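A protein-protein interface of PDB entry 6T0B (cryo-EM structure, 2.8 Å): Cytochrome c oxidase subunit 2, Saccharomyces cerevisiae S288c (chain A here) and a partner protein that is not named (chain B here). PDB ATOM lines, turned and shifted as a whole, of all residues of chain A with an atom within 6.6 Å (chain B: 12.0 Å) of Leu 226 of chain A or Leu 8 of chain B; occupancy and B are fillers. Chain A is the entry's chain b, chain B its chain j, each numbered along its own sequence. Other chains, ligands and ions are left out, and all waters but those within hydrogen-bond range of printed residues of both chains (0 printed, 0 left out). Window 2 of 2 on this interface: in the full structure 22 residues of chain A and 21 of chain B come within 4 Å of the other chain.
O of Ala 99 of chain A lies close to OG1 of Thr 10 of chain B (3.1 Å).
The side-chain hydroxyl (OG1) of Thr 10 of chain B is in hydrogen-bond range of the backbone NH (N) of Met 100 of chain A (3.0 Å).
Of the 9 printed residues of chain B, 4 touch a printed residue of chain A.
Among the printed residues, 8 pairs touch across the chains.
Of the printed residues of chain B, Pro 98 of chain A touches Thr 10 and Val 11.
Ala 99 of chain A touches just these residues of chain B: Leu 8 (3.4 Å) and Thr 10 (3.0 Å).
Printed residues of chain B within 4 Å of Met 100 of chain A: Leu 8 and Thr 10.
Ile 119 of chain A touches just one residue of chain B: Pro 7 (3.9 Å).
No residue of chain B comes within 4 Å of Pro 155 of chain A.
No residue of chain B comes within 4 Å of Val 156 of chain A.
No residue of chain B comes within 4 Å of Thr 158 of chain A.
Leu 226 of chain A touches just one residue of chain B: Leu 8 (3.9 Å).
No residue of chain B comes within 4 Å of Pro 227 of chain A.
Phe 229 of chain A touches none of the printed residues of chain B.
Of the printed residues of chain A, Pro 7 of chain B touches Ile 119 (3.9 Å).
Leu 8 of chain B touches three residues of chain A.
Of the printed residues of chain A, Thr 10 of chain B touches Pro 98 (3.3 Å), Ala 99 (3.0 Å) and Met 100 (3.0 Å).
Of the printed residues of chain A, Val 11 of chain B touches Pro 98.
The nearest residue of chain B that does not touch Leu 226 of chain A is Ser 6 of chain B (4.3 Å).
The nearest residue of chain A that does not touch Leu 8 of chain B is Ile 119 of chain A (4.04 Å).
The nearest printed residue of chain A that does not touch Val 11 of chain B is Ala 99 of chain A (6.5 Å).
N of Leu 8 of chain B lies close to OG of Ser 6 of chain B (3.3 Å).
Among the printed residues, pairs that only touch across the chains: Pro 98 of chain A with Thr 10 of chain B (3.3 Å), Ala 99 of chain A with Leu 8 of chain B (3.4 Å), Pro 98 of chain A with Val 11 of chain B (3.6 Å), Met 100 of chain A with Leu 8 of chain B (3.7 Å), Ile 119 of chain A with Pro 7 of chain B (3.9 Å) and Leu 226 of chain A with Leu 8 of chain B (3.9 Å).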
ATOM      1  N   PRO A  98      -0.053  13.916 -17.470  1.00  0.00           N
ATOM      2  CA  PRO A  98       0.916  14.753 -16.770  1.00  0.00           C
ATOM      3  C   PRO A  98       0.306  15.352 -15.517  1.00  0.00           C
ATOM      4  O   PRO A  98      -0.905  15.535 -15.403  1.00  0.00           O
ATOM      5  CB  PRO A  98       1.251  15.829 -17.799  1.00  0.00           C
ATOM      6  CG  PRO A  98       0.017  15.982 -18.549  1.00  0.00           C
ATOM      7  CD  PRO A  98      -0.678  14.659 -18.577  1.00  0.00           C
ATOM      8  N   ALA A  99       1.174  15.624 -14.553  1.00  0.00           N
ATOM      9  CA  ALA A  99       0.753  16.152 -13.270  1.00  0.00           C
ATOM     10  C   ALA A  99       0.934  17.649 -13.179  1.00  0.00           C
ATOM     11  O   ALA A  99       0.641  18.231 -12.131  1.00  0.00           O
ATOM     12  CB  ALA A  99       1.521  15.471 -12.143  1.00  0.00           C
ATOM     13  N   MET A 100       1.353  18.292 -14.264  1.00  0.00           N
ATOM     14  CA  MET A 100       1.644  19.712 -14.248  1.00  0.00           C
ATOM     15  C   MET A 100       1.731  20.203 -15.677  1.00  0.00           C
ATOM     16  O   MET A 100       2.360  19.558 -16.513  1.00  0.00           O
ATOM     17  CB  MET A 100       2.950  20.004 -13.522  1.00  0.00           C
ATOM     18  CG  MET A 100       3.222  21.460 -13.378  1.00  0.00           C
ATOM     19  SD  MET A 100       4.476  21.760 -12.160  1.00  0.00           S
ATOM     20  CE  MET A 100       3.744  20.818 -10.843  1.00  0.00           C
ATOM     21  N   ILE A 119      -3.745  24.773  -8.668  1.00  0.00           N
ATOM     22  CA  ILE A 119      -3.555  23.899  -7.516  1.00  0.00           C
ATOM     23  C   ILE A 119      -3.237  24.690  -6.260  1.00  0.00           C
ATOM     24  O   ILE A 119      -3.149  24.108  -5.173  1.00  0.00           O
ATOM     25  CB  ILE A 119      -2.445  22.882  -7.834  1.00  0.00           C
ATOM     26  CG1 ILE A 119      -1.139  23.615  -8.134  1.00  0.00           C
ATOM     27  CG2 ILE A 119      -2.846  22.022  -9.023  1.00  0.00           C
ATOM     28  CD1 ILE A 119       0.059  22.710  -8.242  1.00  0.00           C
ATOM     29  N   PRO A 155       8.818  20.590  -9.713  1.00  0.00           N
ATOM     30  CA  PRO A 155       9.083  19.467  -8.817  1.00  0.00           C
ATOM     31  C   PRO A 155       9.692  18.291  -9.555  1.00  0.00           C
ATOM     32  O   PRO A 155       9.577  18.157 -10.771  1.00  0.00           O
ATOM     33  CB  PRO A 155       7.696  19.107  -8.304  1.00  0.00           C
ATOM     34  CG  PRO A 155       6.850  19.397  -9.433  1.00  0.00           C
ATOM     35  CD  PRO A 155       7.398  20.645 -10.068  1.00  0.00           C
ATOM     36  N   VAL A 156      10.329  17.412  -8.795  1.00  0.00           N
ATOM     37  CA  VAL A 156      10.962  16.244  -9.368  1.00  0.00           C
ATOM     38  C   VAL A 156      10.006  15.069  -9.284  1.00  0.00           C
ATOM     39  O   VAL A 156       9.055  15.067  -8.501  1.00  0.00           O
ATOM     40  CB  VAL A 156      12.299  15.912  -8.690  1.00  0.00           C
ATOM     41  CG1 VAL A 156      13.263  17.020  -8.925  1.00  0.00           C
ATOM     42  CG2 VAL A 156      12.092  15.691  -7.211  1.00  0.00           C
ATOM     43  N   ASP A 157      10.276  14.060 -10.120  1.00  0.00           N
ATOM     44  CA  ASP A 157       9.472  12.843 -10.273  1.00  0.00           C
ATOM     45  C   ASP A 157       8.026  13.161 -10.637  1.00  0.00           C
ATOM     46  O   ASP A 157       7.090  12.520 -10.161  1.00  0.00           O
ATOM     47  CB  ASP A 157       9.547  11.956  -9.032  1.00  0.00           C
ATOM     48  CG  ASP A 157      10.905  11.310  -8.869  1.00  0.00           C
ATOM     49  OD1 ASP A 157      11.444  10.804  -9.874  1.00  0.00           O
ATOM     50  OD2 ASP A 157      11.437  11.314  -7.741  1.00  0.00           O
ATOM     51  N   THR A 158       7.849  14.146 -11.508  1.00  0.00           N
ATOM     52  CA  THR A 158       6.537  14.612 -11.917  1.00  0.00           C
ATOM     53  C   THR A 158       6.529  14.766 -13.425  1.00  0.00           C
ATOM     54  O   THR A 158       7.408  15.423 -13.982  1.00  0.00           O
ATOM     55  CB  THR A 158       6.202  15.940 -11.231  1.00  0.00           C
ATOM     56  OG1 THR A 158       5.857  15.696  -9.866  1.00  0.00           O
ATOM     57  CG2 THR A 158       5.049  16.634 -11.908  1.00  0.00           C
ATOM     58  N   VAL A 224      13.152  20.969  -7.784  1.00  0.00           N
ATOM     59  CA  VAL A 224      13.218  20.787  -6.343  1.00  0.00           C
ATOM     60  C   VAL A 224      12.315  19.631  -5.971  1.00  0.00           C
ATOM     61  O   VAL A 224      11.639  19.065  -6.830  1.00  0.00           O
ATOM     62  CB  VAL A 224      12.802  22.067  -5.601  1.00  0.00           C
ATOM     63  CG1 VAL A 224      13.756  23.199  -5.907  1.00  0.00           C
ATOM     64  CG2 VAL A 224      11.409  22.456  -5.995  1.00  0.00           C
ATOM     65  N   SER A 225      12.288  19.265  -4.700  1.00  0.00           N
ATOM     66  CA  SER A 225      11.302  18.288  -4.295  1.00  0.00           C
ATOM     67  C   SER A 225       9.959  18.969  -4.125  1.00  0.00           C
ATOM     68  O   SER A 225       9.863  20.196  -4.073  1.00  0.00           O
ATOM     69  CB  SER A 225      11.704  17.597  -3.005  1.00  0.00           C
ATOM     70  OG  SER A 225      11.662  18.500  -1.925  1.00  0.00           O
ATOM     71  N   LEU A 226       8.916  18.154  -4.032  1.00  0.00           N
ATOM     72  CA  LEU A 226       7.559  18.676  -4.144  1.00  0.00           C
ATOM     73  C   LEU A 226       7.125  19.551  -2.967  1.00  0.00           C
ATOM     74  O   LEU A 226       6.399  20.529  -3.221  1.00  0.00           O
ATOM     75  CB  LEU A 226       6.597  17.506  -4.397  1.00  0.00           C
ATOM     76  CG  LEU A 226       5.153  17.744  -4.816  1.00  0.00           C
ATOM     77  CD1 LEU A 226       4.750  16.692  -5.822  1.00  0.00           C
ATOM     78  CD2 LEU A 226       4.240  17.669  -3.619  1.00  0.00           C
ATOM     79  N   PRO A 227       7.510  19.281  -1.673  1.00  0.00           N
ATOM     80  CA  PRO A 227       7.327  20.298  -0.627  1.00  0.00           C
ATOM     81  C   PRO A 227       7.905  21.672  -0.925  1.00  0.00           C
ATOM     82  O   PRO A 227       7.237  22.692  -0.708  1.00  0.00           O
ATOM     83  CB  PRO A 227       8.050  19.691   0.579  1.00  0.00           C
ATOM     84  CG  PRO A 227       8.275  18.267   0.259  1.00  0.00           C
ATOM     85  CD  PRO A 227       7.663  17.957  -1.043  1.00  0.00           C
ATOM     86  N   LYS A 228       9.143  21.710  -1.408  1.00  0.00           N
ATOM     87  CA  LYS A 228       9.779  22.992  -1.653  1.00  0.00           C
ATOM     88  C   LYS A 228       9.175  23.692  -2.858  1.00  0.00           C
ATOM     89  O   LYS A 228       9.091  24.928  -2.879  1.00  0.00           O
ATOM     90  CB  LYS A 228      11.276  22.801  -1.816  1.00  0.00           C
ATOM     91  CG  LYS A 228      11.908  22.229  -0.569  1.00  0.00           C
ATOM     92  CD  LYS A 228      13.409  22.410  -0.567  1.00  0.00           C
ATOM     93  CE  LYS A 228      13.789  23.869  -0.387  1.00  0.00           C
ATOM     94  NZ  LYS A 228      13.589  24.343   1.011  1.00  0.00           N
ATOM     95  N   PHE A 229       8.708  22.920  -3.839  1.00  0.00           N
ATOM     96  CA  PHE A 229       7.953  23.491  -4.945  1.00  0.00           C
ATOM     97  C   PHE A 229       6.664  24.127  -4.462  1.00  0.00           C
ATOM     98  O   PHE A 229       6.303  25.219  -4.911  1.00  0.00           O
ATOM     99  CB  PHE A 229       7.648  22.412  -5.968  1.00  0.00           C
ATOM    100  CG  PHE A 229       6.735  22.853  -7.055  1.00  0.00           C
ATOM    101  CD1 PHE A 229       7.205  23.626  -8.080  1.00  0.00           C
ATOM    102  CD2 PHE A 229       5.410  22.481  -7.059  1.00  0.00           C
ATOM    103  CE1 PHE A 229       6.377  24.023  -9.081  1.00  0.00           C
ATOM    104  CE2 PHE A 229       4.586  22.890  -8.052  1.00  0.00           C
ATOM    105  CZ  PHE A 229       5.074  23.659  -9.066  1.00  0.00           C
ATOM    106  N   LEU A 230       5.951  23.448  -3.561  1.00  0.00           N
ATOM    107  CA  LEU A 230       4.697  23.984  -3.040  1.00  0.00           C
ATOM    108  C   LEU A 230       4.924  25.255  -2.243  1.00  0.00           C
ATOM    109  O   LEU A 230       4.177  26.229  -2.395  1.00  0.00           O
ATOM    110  CB  LEU A 230       4.000  22.945  -2.170  1.00  0.00           C
ATOM    111  CG  LEU A 230       3.391  21.734  -2.859  1.00  0.00           C
ATOM    112  CD1 LEU A 230       2.577  20.948  -1.863  1.00  0.00           C
ATOM    113  CD2 LEU A 230       2.555  22.135  -4.040  1.00  0.00           C
ATOM    114  N   GLU A 231       5.967  25.281  -1.419  1.00  0.00           N
ATOM    115  CA  GLU A 231       6.219  26.488  -0.646  1.00  0.00           C
ATOM    116  C   GLU A 231       6.769  27.617  -1.513  1.00  0.00           C
ATOM    117  O   GLU A 231       6.665  28.785  -1.128  1.00  0.00           O
ATOM    118  CB  GLU A 231       7.155  26.194   0.522  1.00  0.00           C
ATOM    119  CG  GLU A 231       8.599  26.016   0.156  1.00  0.00           C
ATOM    120  CD  GLU A 231       9.434  25.581   1.330  1.00  0.00           C
ATOM    121  OE1 GLU A 231       8.887  25.508   2.449  1.00  0.00           O
ATOM    122  OE2 GLU A 231      10.631  25.290   1.134  1.00  0.00           O
ATOM    123  N   SER B   6      -1.078  13.093  -4.111  1.00  0.00           N
ATOM    124  CA  SER B   6      -0.650  14.390  -4.621  1.00  0.00           C
ATOM    125  C   SER B   6      -1.838  15.243  -5.031  1.00  0.00           C
ATOM    126  O   SER B   6      -2.756  14.752  -5.684  1.00  0.00           O
ATOM    127  CB  SER B   6       0.291  14.214  -5.808  1.00  0.00           C
ATOM    128  OG  SER B   6       0.641  15.465  -6.359  1.00  0.00           O
ATOM    129  N   PRO B   7      -1.823  16.526  -4.663  1.00  0.00           N
ATOM    130  CA  PRO B   7      -2.887  17.443  -5.086  1.00  0.00           C
ATOM    131  C   PRO B   7      -2.751  17.955  -6.510  1.00  0.00           C
ATOM    132  O   PRO B   7      -3.521  18.835  -6.905  1.00  0.00           O
ATOM    133  CB  PRO B   7      -2.732  18.601  -4.091  1.00  0.00           C
ATOM    134  CG  PRO B   7      -1.278  18.640  -3.836  1.00  0.00           C
ATOM    135  CD  PRO B   7      -0.838  17.202  -3.801  1.00  0.00           C
ATOM    136  N   LEU B   8      -1.805  17.430  -7.281  1.00  0.00           N
ATOM    137  CA  LEU B   8      -1.436  17.971  -8.581  1.00  0.00           C
ATOM    138  C   LEU B   8      -2.262  17.278  -9.653  1.00  0.00           C
ATOM    139  O   LEU B   8      -2.190  16.056  -9.806  1.00  0.00           O
ATOM    140  CB  LEU B   8       0.055  17.773  -8.842  1.00  0.00           C
ATOM    141  CG  LEU B   8       1.124  18.751  -8.353  1.00  0.00           C
ATOM    142  CD1 LEU B   8       1.067  19.044  -6.863  1.00  0.00           C
ATOM    143  CD2 LEU B   8       2.452  18.134  -8.686  1.00  0.00           C
ATOM    144  N   HIS B   9      -3.048  18.057 -10.383  1.00  0.00           N
ATOM    145  CA  HIS B   9      -3.920  17.528 -11.414  1.00  0.00           C
ATOM    146  C   HIS B   9      -3.925  18.496 -12.580  1.00  0.00           C
ATOM    147  O   HIS B   9      -3.843  19.714 -12.393  1.00  0.00           O
ATOM    148  CB  HIS B   9      -5.339  17.302 -10.886  1.00  0.00           C
ATOM    149  CG  HIS B   9      -5.457  16.104  -9.995  1.00  0.00           C
ATOM    150  ND1 HIS B   9      -4.588  15.036 -10.067  1.00  0.00           N
ATOM    151  CD2 HIS B   9      -6.337  15.805  -9.011  1.00  0.00           C
ATOM    152  CE1 HIS B   9      -4.927  14.131  -9.168  1.00  0.00           C
ATOM    153  NE2 HIS B   9      -5.986  14.573  -8.513  1.00  0.00           N
ATOM    154  N   THR B  10      -3.999  17.944 -13.783  1.00  0.00           N
ATOM    155  CA  THR B  10      -3.747  18.677 -15.012  1.00  0.00           C
ATOM    156  C   THR B  10      -4.674  18.104 -16.072  1.00  0.00           C
ATOM    157  O   THR B  10      -5.266  17.041 -15.875  1.00  0.00           O
ATOM    158  CB  THR B  10      -2.248  18.557 -15.362  1.00  0.00           C
ATOM    159  OG1 THR B  10      -1.498  19.051 -14.260  1.00  0.00           O
ATOM    160  CG2 THR B  10      -1.796  19.357 -16.564  1.00  0.00           C
ATOM    161  N   VAL B  11      -4.888  18.873 -17.141  1.00  0.00           N
ATOM    162  CA  VAL B  11      -5.428  18.354 -18.388  1.00  0.00           C
ATOM    163  C   VAL B  11      -4.705  17.073 -18.803  1.00  0.00           C
ATOM    164  O   VAL B  11      -3.473  16.995 -18.823  1.00  0.00           O
ATOM    165  CB  VAL B  11      -5.352  19.453 -19.466  1.00  0.00           C
ATOM    166  CG1 VAL B  11      -3.934  19.991 -19.637  1.00  0.00           C
ATOM    167  CG2 VAL B  11      -5.886  18.966 -20.778  1.00  0.00           C
ATOM    168  N   GLY B  12      -5.472  16.042 -19.063  1.00  0.00           N
ATOM    169  CA  GLY B  12      -4.916  14.857 -19.673  1.00  0.00           C
ATOM    170  C   GLY B  12      -4.910  14.970 -21.181  1.00  0.00           C
ATOM    171  O   GLY B  12      -5.486  15.887 -21.754  1.00  0.00           O
ATOM    172  N   LYS B  52     -11.100  24.653 -17.234  1.00  0.00           N
ATOM    173  CA  LYS B  52      -9.770  24.201 -16.835  1.00  0.00           C
ATOM    174  C   LYS B  52      -8.929  23.849 -18.055  1.00  0.00           C
ATOM    175  O   LYS B  52      -7.729  24.144 -18.084  1.00  0.00           O
ATOM    176  CB  LYS B  52      -9.856  23.027 -15.840  1.00  0.00           C
ATOM    177  CG  LYS B  52     -10.498  21.714 -16.310  1.00  0.00           C
ATOM    178  CD  LYS B  52      -9.496  20.690 -16.873  1.00  0.00           C
ATOM    179  CE  LYS B  52     -10.189  19.415 -17.339  1.00  0.00           C
ATOM    180  NZ  LYS B  52      -9.251  18.440 -17.966  1.00  0.00           N
ATOM    181  N   ALA B  56      -5.690  26.161 -18.715  1.00  0.00           N
ATOM    182  CA  ALA B  56      -4.463  25.485 -18.319  1.00  0.00           C
ATOM    183  C   ALA B  56      -3.409  25.528 -19.414  1.00  0.00           C
ATOM    184  O   ALA B  56      -2.211  25.566 -19.117  1.00  0.00           O
ATOM    185  CB  ALA B  56      -4.766  24.039 -17.931  1.00  0.00           C
